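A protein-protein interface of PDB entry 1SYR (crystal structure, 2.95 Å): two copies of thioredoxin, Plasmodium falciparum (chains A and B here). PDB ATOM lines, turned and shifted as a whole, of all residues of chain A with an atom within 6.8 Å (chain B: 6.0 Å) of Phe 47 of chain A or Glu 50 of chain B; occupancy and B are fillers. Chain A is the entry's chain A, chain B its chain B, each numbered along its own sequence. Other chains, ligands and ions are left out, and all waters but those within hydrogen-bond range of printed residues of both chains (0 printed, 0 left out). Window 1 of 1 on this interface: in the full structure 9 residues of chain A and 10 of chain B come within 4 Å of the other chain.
The side-chain hydroxyl of Thr 54 of chain B sits at hydrogen-bond distance from the side-chain carboxylate of Glu 50 of chain A (2.9 Å).
The side-chain amino group (NZ) of Lys 53 of chain B sits at hydrogen-bond distance from the side-chain hydroxyl (OH) of Tyr 55 of chain A, 3.5 Å away.
The side-chain amino group of Lys 104 of chain A is in salt-bridge range of the side-chain carboxylate of Glu 49 of chain B (3.7 Å).
The side-chain carboxylate of Asp 100 of chain A lies close to the side-chain carboxylate of Asp 100 of chain B (3.0 Å).
The backbone carbonyl oxygen of Phe 47 of chain A sits at hydrogen-bond distance from the side-chain sulfur of Cys 51 of chain A (3.3 Å).
The backbone carbonyl oxygen of Phe 47 of chain B is in hydrogen-bond range of the side-chain sulfur of Cys 51 of chain B, 3.5 Å away.
The backbone carbonyl oxygen (O) of Glu 49 of chain B lies within hydrogen-bond range of the side-chain hydroxyl (OG) of Ser 52 of chain B.
O of Cys 51 of chain B is in hydrogen-bond range of OG1 of Thr 54 of chain B (3.4 Å).
Pro 46 of chain A touches Phe 47 of chain B (O to CE1, 3.8 Å).
Phe 47 of chain A touches Pro 46 of chain B (CE1 to O, 3.7 Å).
CD1 of Phe 47 of chain A touches CD1 of Phe 47 of chain B (3.6 Å).
Glu 50 of chain B touches Phe 47 of chain A (CG to CE1, 3.8 Å).
OE2 of Glu 50 of chain A touches CE2 of Tyr 55 of chain B, 3.6 Å away.
SG of Cys 51 of chain A touches CG of Glu 50 of chain B, 3.8 Å away.
CG2 of Thr 54 of chain A touches OE2 of Glu 50 of chain B (2.9 Å).
Thr 54 of chain B touches Thr 54 of chain A.
Glu 50 of chain B touches Tyr 55 of chain A (OE2 to CE2, 3.9 Å).
Asp 100 of chain A touches Phe 47 of chain B.
Glu 50 of chain A touches Cys 51 of chain B, and with the chains exchanged Cys 51 of chain A touches Glu 50 of chain B.
Glu 50 of chain A touches Tyr 55 of chain B, and with the chains exchanged Tyr 55 of chain A touches Glu 50 of chain B.
Thr 54 of chain A touches its own counterpart, Thr 54 of chain B.
Asp 100 of chain B touches its own counterpart, Asp 100 of chain A.
11 positions are printed for both chains.
Phe 47 of chain A touches just these residues of chain B: Pro 46 (3.7 Å), Phe 47 (3.6 Å), Glu 50 (3.8 Å) and Asp 100 (3.96 Å).
Of the printed residues of chain B, Glu 50 of chain A touches Cys 51 (3.9 Å), Thr 54 (2.9 Å) and Tyr 55 (3.6 Å).
Printed residues of chain B within 4 Å of Tyr 55 of chain A: Glu 50 (3.9 Å) and Lys 53 (3.5 Å).
Ala 102 of chain A touches none of the printed residues of chain B.
Of the printed residues of chain A, Pro 46 of chain B touches Phe 47 (3.7 Å).
Of chain A, only Phe 47, Cys 51, Thr 54, Tyr 55 and Lys 104 come within 4 Å of Glu 50 of chain B.
Printed residues of chain A within 4 Å of Lys 53 of chain B: Tyr 55 (3.5 Å).
Of the printed residues of chain A, Asp 100 of chain B touches Phe 47 and Asp 100.
The nearest printed residue of chain B that does not touch Phe 47 of chain A is Tyr 48 of chain B (6.0 Å).
The nearest printed residue of chain A that does not touch Glu 49 of chain B is Phe 47 of chain A (6.7 Å).
Of the 22 printed residues of chain A, 8 touch a printed residue of chain B.
Printed residues of chain A that touch a printed residue of chain B: Pro 46, Phe 47, Glu 50, Cys 51, Thr 54, Tyr 55, Asp 100 and Lys 104.
Hydrophobic or aromatic side chains of chain A that line the printed part of chain B: Phe 47 and Tyr 55.
Hydrophobic or aromatic side chains of chain B that line the printed part of chain A: Phe 47 and Tyr 55.
Along chain B the printed residues that touch a printed residue of chain A span positions 46 to 100.
Among the printed residues, Asp or Glu carboxylates within 4 Å of a Lys or Arg side-chain nitrogen of the other chain: Lys 104 of chain A with Glu 49 of chain B (3.7 Å).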
ATOM      1  N   ARG A  43      24.243  11.701   2.291  1.00  0.00           N
ATOM      2  CA  ARG A  43      23.081  12.587   2.420  1.00  0.00           C
ATOM      3  C   ARG A  43      21.910  12.096   1.571  1.00  0.00           C
ATOM      4  O   ARG A  43      20.753  12.119   2.004  1.00  0.00           O
ATOM      5  CB  ARG A  43      23.442  14.021   2.022  1.00  0.00           C
ATOM      6  CG  ARG A  43      23.623  14.986   3.194  1.00  0.00           C
ATOM      7  CD  ARG A  43      24.339  16.297   2.829  1.00  0.00           C
ATOM      8  NE  ARG A  43      25.780  16.103   2.620  1.00  0.00           N
ATOM      9  CZ  ARG A  43      26.730  16.974   2.972  1.00  0.00           C
ATOM     10  NH1 ARG A  43      26.406  18.126   3.557  1.00  0.00           N
ATOM     11  NH2 ARG A  43      28.010  16.694   2.737  1.00  0.00           N
ATOM     12  N   ILE A  44      22.214  11.638   0.364  1.00  0.00           N
ATOM     13  CA  ILE A  44      21.173  11.274  -0.583  1.00  0.00           C
ATOM     14  C   ILE A  44      20.682   9.835  -0.442  1.00  0.00           C
ATOM     15  O   ILE A  44      19.665   9.470  -1.033  1.00  0.00           O
ATOM     16  CB  ILE A  44      21.629  11.579  -2.026  1.00  0.00           C
ATOM     17  CG1 ILE A  44      20.425  11.588  -2.969  1.00  0.00           C
ATOM     18  CG2 ILE A  44      22.729  10.613  -2.490  1.00  0.00           C
ATOM     19  CD1 ILE A  44      20.392  12.742  -3.888  1.00  0.00           C
ATOM     20  N   ALA A  45      21.391   9.033   0.354  1.00  0.00           N
ATOM     21  CA  ALA A  45      20.993   7.648   0.631  1.00  0.00           C
ATOM     22  C   ALA A  45      19.513   7.463   1.054  1.00  0.00           C
ATOM     23  O   ALA A  45      18.816   6.660   0.441  1.00  0.00           O
ATOM     24  CB  ALA A  45      21.947   6.996   1.644  1.00  0.00           C
ATOM     25  N   PRO A  46      19.016   8.190   2.062  1.00  0.00           N
ATOM     26  CA  PRO A  46      17.633   7.988   2.502  1.00  0.00           C
ATOM     27  C   PRO A  46      16.610   8.269   1.399  1.00  0.00           C
ATOM     28  O   PRO A  46      15.610   7.556   1.337  1.00  0.00           O
ATOM     29  CB  PRO A  46      17.483   8.985   3.657  1.00  0.00           C
ATOM     30  CG  PRO A  46      18.860   9.201   4.122  1.00  0.00           C
ATOM     31  CD  PRO A  46      19.674   9.238   2.863  1.00  0.00           C
ATOM     32  N   PHE A  47      16.861   9.262   0.545  1.00  0.00           N
ATOM     33  CA  PHE A  47      15.961   9.552  -0.570  1.00  0.00           C
ATOM     34  C   PHE A  47      15.931   8.405  -1.585  1.00  0.00           C
ATOM     35  O   PHE A  47      14.864   8.002  -2.051  1.00  0.00           O
ATOM     36  CB  PHE A  47      16.341  10.873  -1.257  1.00  0.00           C
ATOM     37  CG  PHE A  47      15.387  11.285  -2.349  1.00  0.00           C
ATOM     38  CD1 PHE A  47      14.048  11.534  -2.073  1.00  0.00           C
ATOM     39  CD2 PHE A  47      15.825  11.412  -3.658  1.00  0.00           C
ATOM     40  CE1 PHE A  47      13.172  11.896  -3.084  1.00  0.00           C
ATOM     41  CE2 PHE A  47      14.943  11.778  -4.675  1.00  0.00           C
ATOM     42  CZ  PHE A  47      13.622  12.020  -4.383  1.00  0.00           C
ATOM     43  N   TYR A  48      17.111   7.891  -1.916  1.00  0.00           N
ATOM     44  CA  TYR A  48      17.258   6.749  -2.812  1.00  0.00           C
ATOM     45  C   TYR A  48      16.532   5.523  -2.262  1.00  0.00           C
ATOM     46  O   TYR A  48      15.847   4.836  -3.019  1.00  0.00           O
ATOM     47  CB  TYR A  48      18.744   6.443  -3.031  1.00  0.00           C
ATOM     48  CG  TYR A  48      19.080   5.460  -4.135  1.00  0.00           C
ATOM     49  CD1 TYR A  48      18.900   5.789  -5.474  1.00  0.00           C
ATOM     50  CD2 TYR A  48      19.629   4.206  -3.835  1.00  0.00           C
ATOM     51  CE1 TYR A  48      19.231   4.889  -6.490  1.00  0.00           C
ATOM     52  CE2 TYR A  48      19.964   3.291  -4.846  1.00  0.00           C
ATOM     53  CZ  TYR A  48      19.761   3.643  -6.165  1.00  0.00           C
ATOM     54  OH  TYR A  48      20.098   2.755  -7.156  1.00  0.00           O
ATOM     55  N   GLU A  49      16.665   5.253  -0.957  1.00  0.00           N
ATOM     56  CA  GLU A  49      15.995   4.098  -0.355  1.00  0.00           C
ATOM     57  C   GLU A  49      14.490   4.280  -0.420  1.00  0.00           C
ATOM     58  O   GLU A  49      13.755   3.335  -0.722  1.00  0.00           O
ATOM     59  CB  GLU A  49      16.434   3.848   1.093  1.00  0.00           C
ATOM     60  CG  GLU A  49      15.961   2.502   1.656  1.00  0.00           C
ATOM     61  CD  GLU A  49      17.100   1.514   1.907  1.00  0.00           C
ATOM     62  OE1 GLU A  49      18.257   1.777   1.467  1.00  0.00           O
ATOM     63  OE2 GLU A  49      16.833   0.464   2.551  1.00  0.00           O
ATOM     64  N   GLU A  50      14.042   5.503  -0.147  1.00  0.00           N
ATOM     65  CA  GLU A  50      12.628   5.827  -0.232  1.00  0.00           C
ATOM     66  C   GLU A  50      12.107   5.613  -1.640  1.00  0.00           C
ATOM     67  O   GLU A  50      11.116   4.923  -1.830  1.00  0.00           O
ATOM     68  CB  GLU A  50      12.362   7.257   0.225  1.00  0.00           C
ATOM     69  CG  GLU A  50      11.076   7.422   1.010  1.00  0.00           C
ATOM     70  CD  GLU A  50      10.941   6.407   2.126  1.00  0.00           C
ATOM     71  OE1 GLU A  50      11.879   6.299   2.944  1.00  0.00           O
ATOM     72  OE2 GLU A  50       9.899   5.715   2.182  1.00  0.00           O
ATOM     73  N   CYS A  51      12.791   6.182  -2.627  1.00  0.00           N
ATOM     74  CA  CYS A  51      12.373   6.039  -4.019  1.00  0.00           C
ATOM     75  C   CYS A  51      12.245   4.578  -4.446  1.00  0.00           C
ATOM     76  O   CYS A  51      11.340   4.224  -5.202  1.00  0.00           O
ATOM     77  CB  CYS A  51      13.331   6.781  -4.943  1.00  0.00           C
ATOM     78  SG  CYS A  51      13.163   8.573  -4.858  1.00  0.00           S
ATOM     79  N   SER A  52      13.143   3.733  -3.946  1.00  0.00           N
ATOM     80  CA  SER A  52      13.127   2.317  -4.285  1.00  0.00           C
ATOM     81  C   SER A  52      11.821   1.653  -3.833  1.00  0.00           C
ATOM     82  O   SER A  52      11.340   0.720  -4.481  1.00  0.00           O
ATOM     83  CB  SER A  52      14.358   1.595  -3.714  1.00  0.00           C
ATOM     84  OG  SER A  52      14.140   1.124  -2.397  1.00  0.00           O
ATOM     85  N   THR A  54       8.819   3.031  -3.795  1.00  0.00           N
ATOM     86  CA  THR A  54       7.672   3.482  -4.586  1.00  0.00           C
ATOM     87  C   THR A  54       7.793   3.221  -6.094  1.00  0.00           C
ATOM     88  O   THR A  54       6.858   2.698  -6.703  1.00  0.00           O
ATOM     89  CB  THR A  54       7.359   4.970  -4.296  1.00  0.00           C
ATOM     90  OG1 THR A  54       6.763   5.574  -5.450  1.00  0.00           O
ATOM     91  CG2 THR A  54       8.642   5.779  -4.094  1.00  0.00           C
ATOM     92  N   TYR A  55       8.928   3.579  -6.693  1.00  0.00           N
ATOM     93  CA  TYR A  55       9.160   3.336  -8.120  1.00  0.00           C
ATOM     94  C   TYR A  55       9.558   1.876  -8.378  1.00  0.00           C
ATOM     95  O   TYR A  55      10.692   1.570  -8.764  1.00  0.00           O
ATOM     96  CB  TYR A  55      10.203   4.318  -8.667  1.00  0.00           C
ATOM     97  CG  TYR A  55       9.738   5.764  -8.667  1.00  0.00           C
ATOM     98  CD1 TYR A  55       8.617   6.159  -9.397  1.00  0.00           C
ATOM     99  CD2 TYR A  55      10.417   6.737  -7.933  1.00  0.00           C
ATOM    100  CE1 TYR A  55       8.186   7.488  -9.397  1.00  0.00           C
ATOM    101  CE2 TYR A  55       9.997   8.069  -7.928  1.00  0.00           C
ATOM    102  CZ  TYR A  55       8.882   8.435  -8.662  1.00  0.00           C
ATOM    103  OH  TYR A  55       8.456   9.743  -8.659  1.00  0.00           O
ATOM    104  N   PHE A  60      16.650  -1.088  -7.739  1.00  0.00           N
ATOM    105  CA  PHE A  60      17.656  -0.173  -7.217  1.00  0.00           C
ATOM    106  C   PHE A  60      18.817  -0.943  -6.589  1.00  0.00           C
ATOM    107  O   PHE A  60      18.601  -1.754  -5.692  1.00  0.00           O
ATOM    108  CB  PHE A  60      17.039   0.737  -6.147  1.00  0.00           C
ATOM    109  CG  PHE A  60      16.107   1.812  -6.684  1.00  0.00           C
ATOM    110  CD1 PHE A  60      15.049   1.500  -7.537  1.00  0.00           C
ATOM    111  CD2 PHE A  60      16.273   3.143  -6.294  1.00  0.00           C
ATOM    112  CE1 PHE A  60      14.199   2.494  -8.015  1.00  0.00           C
ATOM    113  CE2 PHE A  60      15.418   4.144  -6.764  1.00  0.00           C
ATOM    114  CZ  PHE A  60      14.383   3.818  -7.626  1.00  0.00           C
ATOM    115  N   ASN A  99      21.614  15.506  -5.883  1.00  0.00           N
ATOM    116  CA  ASN A  99      20.464  16.399  -5.846  1.00  0.00           C
ATOM    117  C   ASN A  99      19.140  15.638  -5.870  1.00  0.00           C
ATOM    118  O   ASN A  99      18.799  15.012  -6.873  1.00  0.00           O
ATOM    119  CB  ASN A  99      20.539  17.381  -7.006  1.00  0.00           C
ATOM    120  CG  ASN A  99      19.534  18.484  -6.884  1.00  0.00           C
ATOM    121  OD1 ASN A  99      18.396  18.349  -7.319  1.00  0.00           O
ATOM    122  ND2 ASN A  99      19.942  19.586  -6.278  1.00  0.00           N
ATOM    123  N   ASP A 100      18.403  15.694  -4.764  1.00  0.00           N
ATOM    124  CA  ASP A 100      17.086  15.057  -4.652  1.00  0.00           C
ATOM    125  C   ASP A 100      16.153  15.323  -5.839  1.00  0.00           C
ATOM    126  O   ASP A 100      15.627  14.390  -6.450  1.00  0.00           O
ATOM    127  CB  ASP A 100      16.388  15.524  -3.374  1.00  0.00           C
ATOM    128  CG  ASP A 100      16.862  14.782  -2.151  1.00  0.00           C
ATOM    129  OD1 ASP A 100      18.035  14.342  -2.136  1.00  0.00           O
ATOM    130  OD2 ASP A 100      16.125  14.604  -1.155  1.00  0.00           O
ATOM    131  N   SER A 101      15.946  16.600  -6.151  1.00  0.00           N
ATOM    132  CA  SER A 101      15.091  16.990  -7.264  1.00  0.00           C
ATOM    133  C   SER A 101      15.525  16.360  -8.593  1.00  0.00           C
ATOM    134  O   SER A 101      14.690  15.898  -9.377  1.00  0.00           O
ATOM    135  CB  SER A 101      15.053  18.510  -7.387  1.00  0.00           C
ATOM    136  OG  SER A 101      13.925  18.904  -8.127  1.00  0.00           O
ATOM    137  N   ALA A 102      16.833  16.344  -8.830  1.00  0.00           N
ATOM    138  CA  ALA A 102      17.391  15.829 -10.072  1.00  0.00           C
ATOM    139  C   ALA A 102      17.265  14.312 -10.154  1.00  0.00           C
ATOM    140  O   ALA A 102      16.868  13.779 -11.196  1.00  0.00           O
ATOM    141  CB  ALA A 102      18.836  16.257 -10.218  1.00  0.00           C
ATOM    142  N   LEU A 103      17.598  13.633  -9.050  1.00  0.00           N
ATOM    143  CA  LEU A 103      17.514  12.171  -8.941  1.00  0.00           C
ATOM    144  C   LEU A 103      16.091  11.678  -9.156  1.00  0.00           C
ATOM    145  O   LEU A 103      15.885  10.666  -9.830  1.00  0.00           O
ATOM    146  CB  LEU A 103      18.043  11.689  -7.583  1.00  0.00           C
ATOM    147  CG  LEU A 103      17.949  10.214  -7.149  1.00  0.00           C
ATOM    148  CD1 LEU A 103      18.545   9.260  -8.180  1.00  0.00           C
ATOM    149  CD2 LEU A 103      18.612  10.022  -5.797  1.00  0.00           C
ATOM    150  N   LYS A 104      15.124  12.400  -8.579  1.00  0.00           N
ATOM    151  CA  LYS A 104      13.706  12.117  -8.768  1.00  0.00           C
ATOM    152  C   LYS A 104      13.406  12.147 -10.253  1.00  0.00           C
ATOM    153  O   LYS A 104      12.801  11.219 -10.786  1.00  0.00           O
ATOM    154  CB  LYS A 104      12.849  13.149  -8.032  1.00  0.00           C
ATOM    155  CG  LYS A 104      11.413  12.708  -7.735  1.00  0.00           C
ATOM    156  CD  LYS A 104      10.482  13.920  -7.591  1.00  0.00           C
ATOM    157  CE  LYS A 104       9.203  13.599  -6.813  1.00  0.00           C
ATOM    158  NZ  LYS A 104       8.287  14.784  -6.755  1.00  0.00           N
ATOM    159  N   GLN A 105      13.873  13.208 -10.909  1.00  0.00           N
ATOM    160  CA  GLN A 105      13.644  13.430 -12.333  1.00  0.00           C
ATOM    161  C   GLN A 105      14.177  12.274 -13.178  1.00  0.00           C
ATOM    162  O   GLN A 105      13.491  11.790 -14.080  1.00  0.00           O
ATOM    163  CB  GLN A 105      14.279  14.749 -12.774  1.00  0.00           C
ATOM    164  CG  GLN A 105      13.402  15.961 -12.563  1.00  0.00           C
ATOM    165  CD  GLN A 105      13.417  16.896 -13.757  1.00  0.00           C
ATOM    166  OE1 GLN A 105      14.484  17.232 -14.270  1.00  0.00           O
ATOM    167  NE2 GLN A 105      12.235  17.320 -14.202  1.00  0.00           N
ATOM    168  N   ILE A 107      14.786   9.110 -12.149  1.00  0.00           N
ATOM    169  CA  ILE A 107      13.985   7.921 -11.859  1.00  0.00           C
ATOM    170  C   ILE A 107      12.620   7.985 -12.564  1.00  0.00           C
ATOM    171  O   ILE A 107      12.177   6.996 -13.162  1.00  0.00           O
ATOM    172  CB  ILE A 107      13.810   7.722 -10.336  1.00  0.00           C
ATOM    173  CG1 ILE A 107      15.164   7.622  -9.645  1.00  0.00           C
ATOM    174  CG2 ILE A 107      13.027   6.453 -10.049  1.00  0.00           C
ATOM    175  CD1 ILE A 107      15.101   7.789  -8.139  1.00  0.00           C
ATOM    176  N   GLU A 108      11.978   9.154 -12.503  1.00  0.00           N
ATOM    177  CA  GLU A 108      10.657   9.366 -13.103  1.00  0.00           C
ATOM    178  C   GLU A 108      10.673   9.206 -14.618  1.00  0.00           C
ATOM    179  O   GLU A 108       9.661   8.843 -15.220  1.00  0.00           O
ATOM    180  CB  GLU A 108      10.097  10.736 -12.718  1.00  0.00           C
ATOM    181  CG  GLU A 108       8.965  10.655 -11.711  1.00  0.00           C
ATOM    182  CD  GLU A 108       8.464  12.015 -11.276  1.00  0.00           C
ATOM    183  OE1 GLU A 108       9.148  12.678 -10.472  1.00  0.00           O
ATOM    184  OE2 GLU A 108       7.377  12.418 -11.738  1.00  0.00           O
ATOM    185  N   ALA B  45      11.684  19.296  -0.126  1.00  0.00           N
ATOM    186  CA  ALA B  45      10.332  19.107  -0.629  1.00  0.00           C
ATOM    187  C   ALA B  45      10.181  17.783  -1.387  1.00  0.00           C
ATOM    188  O   ALA B  45       9.279  17.014  -1.062  1.00  0.00           O
ATOM    189  CB  ALA B  45       9.880  20.290  -1.465  1.00  0.00           C
ATOM    190  N   PRO B  46      11.057  17.481  -2.355  1.00  0.00           N
ATOM    191  CA  PRO B  46      10.942  16.217  -3.102  1.00  0.00           C
ATOM    192  C   PRO B  46      10.937  14.963  -2.209  1.00  0.00           C
ATOM    193  O   PRO B  46      10.203  14.012  -2.501  1.00  0.00           O
ATOM    194  CB  PRO B  46      12.171  16.238  -4.020  1.00  0.00           C
ATOM    195  CG  PRO B  46      12.491  17.674  -4.179  1.00  0.00           C
ATOM    196  CD  PRO B  46      12.201  18.286  -2.832  1.00  0.00           C
ATOM    197  N   PHE B  47      11.729  14.973  -1.138  1.00  0.00           N
ATOM    198  CA  PHE B  47      11.765  13.858  -0.199  1.00  0.00           C
ATOM    199  C   PHE B  47      10.443  13.752   0.536  1.00  0.00           C
ATOM    200  O   PHE B  47       9.922  12.653   0.721  1.00  0.00           O
ATOM    201  CB  PHE B  47      12.918  14.012   0.793  1.00  0.00           C
ATOM    202  CG  PHE B  47      13.005  12.900   1.814  1.00  0.00           C
ATOM    203  CD1 PHE B  47      13.460  11.639   1.455  1.00  0.00           C
ATOM    204  CD2 PHE B  47      12.647  13.127   3.142  1.00  0.00           C
ATOM    205  CE1 PHE B  47      13.552  10.612   2.405  1.00  0.00           C
ATOM    206  CE2 PHE B  47      12.732  12.112   4.093  1.00  0.00           C
ATOM    207  CZ  PHE B  47      13.183  10.855   3.725  1.00  0.00           C
ATOM    208  N   TYR B  48       9.905  14.896   0.950  1.00  0.00           N
ATOM    209  CA  TYR B  48       8.609  14.942   1.608  1.00  0.00           C
ATOM    210  C   TYR B  48       7.528  14.391   0.676  1.00  0.00           C
ATOM    211  O   TYR B  48       6.770  13.506   1.065  1.00  0.00           O
ATOM    212  CB  TYR B  48       8.303  16.371   2.049  1.00  0.00           C
ATOM    213  CG  TYR B  48       7.125  16.540   2.989  1.00  0.00           C
ATOM    214  CD1 TYR B  48       7.193  16.134   4.322  1.00  0.00           C
ATOM    215  CD2 TYR B  48       5.949  17.142   2.548  1.00  0.00           C
ATOM    216  CE1 TYR B  48       6.105  16.310   5.188  1.00  0.00           C
ATOM    217  CE2 TYR B  48       4.857  17.327   3.405  1.00  0.00           C
ATOM    218  CZ  TYR B  48       4.941  16.910   4.717  1.00  0.00           C
ATOM    219  OH  TYR B  48       3.858  17.110   5.539  1.00  0.00           O
ATOM    220  N   GLU B  49       7.487  14.889  -0.559  1.00  0.00           N
ATOM    221  CA  GLU B  49       6.564  14.394  -1.577  1.00  0.00           C
ATOM    222  C   GLU B  49       6.644  12.880  -1.678  1.00  0.00           C
ATOM    223  O   GLU B  49       5.619  12.200  -1.742  1.00  0.00           O
ATOM    224  CB  GLU B  49       6.893  15.014  -2.936  1.00  0.00           C
ATOM    225  CG  GLU B  49       5.719  15.051  -3.907  1.00  0.00           C
ATOM    226  CD  GLU B  49       5.370  16.467  -4.355  1.00  0.00           C
ATOM    227  OE1 GLU B  49       5.099  17.345  -3.486  1.00  0.00           O
ATOM    228  OE2 GLU B  49       5.360  16.701  -5.587  1.00  0.00           O
ATOM    229  N   GLU B  50       7.877  12.369  -1.683  1.00  0.00           N
ATOM    230  CA  GLU B  50       8.156  10.945  -1.804  1.00  0.00           C
ATOM    231  C   GLU B  50       7.602  10.113  -0.655  1.00  0.00           C
ATOM    232  O   GLU B  50       7.039   9.046  -0.872  1.00  0.00           O
ATOM    233  CB  GLU B  50       9.666  10.714  -1.913  1.00  0.00           C
ATOM    234  CG  GLU B  50      10.056   9.645  -2.914  1.00  0.00           C
ATOM    235  CD  GLU B  50       9.175   9.682  -4.144  1.00  0.00           C
ATOM    236  OE1 GLU B  50       9.141  10.740  -4.822  1.00  0.00           O
ATOM    237  OE2 GLU B  50       8.500   8.665  -4.416  1.00  0.00           O
ATOM    238  N   CYS B  51       7.786  10.602   0.565  1.00  0.00           N
ATOM    239  CA  CYS B  51       7.358   9.886   1.755  1.00  0.00           C
ATOM    240  C   CYS B  51       5.839   9.805   1.816  1.00  0.00           C
ATOM    241  O   CYS B  51       5.273   8.778   2.210  1.00  0.00           O
ATOM    242  CB  CYS B  51       7.910  10.573   2.998  1.00  0.00           C
ATOM    243  SG  CYS B  51       9.661  10.225   3.267  1.00  0.00           S
ATOM    244  N   SER B  52       5.188  10.891   1.406  1.00  0.00           N
ATOM    245  CA  SER B  52       3.736  10.972   1.378  1.00  0.00           C
ATOM    246  C   SER B  52       3.149   9.882   0.490  1.00  0.00           C
ATOM    247  O   SER B  52       1.980   9.514   0.647  1.00  0.00           O
ATOM    248  CB  SER B  52       3.301  12.340   0.884  1.00  0.00           C
ATOM    249  OG  SER B  52       3.306  12.375  -0.523  1.00  0.00           O
ATOM    250  N   LYS B  53       3.967   9.371  -0.435  1.00  0.00           N
ATOM    251  CA  LYS B  53       3.553   8.304  -1.345  1.00  0.00           C
ATOM    252  C   LYS B  53       3.610   6.950  -0.673  1.00  0.00           C
ATOM    253  O   LYS B  53       2.743   6.115  -0.908  1.00  0.00           O
ATOM    254  CB  LYS B  53       4.389   8.301  -2.633  1.00  0.00           C
ATOM    255  CG  LYS B  53       3.990   9.400  -3.614  1.00  0.00           C
ATOM    256  CD  LYS B  53       4.701   9.279  -4.953  1.00  0.00           C
ATOM    257  CE  LYS B  53       4.657  10.612  -5.714  1.00  0.00           C
ATOM    258  NZ  LYS B  53       5.641  10.666  -6.841  1.00  0.00           N
ATOM    259  N   THR B  54       4.612   6.731   0.172  1.00  0.00           N
ATOM    260  CA  THR B  54       4.777   5.414   0.796  1.00  0.00           C
ATOM    261  C   THR B  54       4.075   5.287   2.142  1.00  0.00           C
ATOM    262  O   THR B  54       3.563   4.211   2.467  1.00  0.00           O
ATOM    263  CB  THR B  54       6.270   4.969   0.901  1.00  0.00           C
ATOM    264  OG1 THR B  54       7.009   5.886   1.713  1.00  0.00           O
ATOM    265  CG2 THR B  54       6.964   5.057  -0.451  1.00  0.00           C
ATOM    266  N   TYR B  55       4.040   6.372   2.914  1.00  0.00           N
ATOM    267  CA  TYR B  55       3.483   6.328   4.264  1.00  0.00           C
ATOM    268  C   TYR B  55       2.006   6.710   4.248  1.00  0.00           C
ATOM    269  O   TYR B  55       1.604   7.754   4.782  1.00  0.00           O
ATOM    270  CB  TYR B  55       4.314   7.193   5.222  1.00  0.00           C
ATOM    271  CG  TYR B  55       5.706   6.634   5.447  1.00  0.00           C
ATOM    272  CD1 TYR B  55       5.889   5.437   6.150  1.00  0.00           C
ATOM    273  CD2 TYR B  55       6.840   7.273   4.936  1.00  0.00           C
ATOM    274  CE1 TYR B  55       7.161   4.897   6.353  1.00  0.00           C
ATOM    275  CE2 TYR B  55       8.126   6.740   5.137  1.00  0.00           C
ATOM    276  CZ  TYR B  55       8.274   5.547   5.848  1.00  0.00           C
ATOM    277  OH  TYR B  55       9.522   4.989   6.063  1.00  0.00           O
ATOM    278  N   ASP B 100      16.999  14.891   5.800  1.00  0.00           N
ATOM    279  CA  ASP B 100      16.266  13.754   5.245  1.00  0.00           C
ATOM    280  C   ASP B 100      16.080  12.612   6.241  1.00  0.00           C
ATOM    281  O   ASP B 100      14.951  12.201   6.510  1.00  0.00           O
ATOM    282  CB  ASP B 100      16.964  13.244   3.975  1.00  0.00           C
ATOM    283  CG  ASP B 100      16.507  13.970   2.712  1.00  0.00           C
ATOM    284  OD1 ASP B 100      15.781  14.986   2.807  1.00  0.00           O
ATOM    285  OD2 ASP B 100      16.842  13.593   1.572  1.00  0.00           O
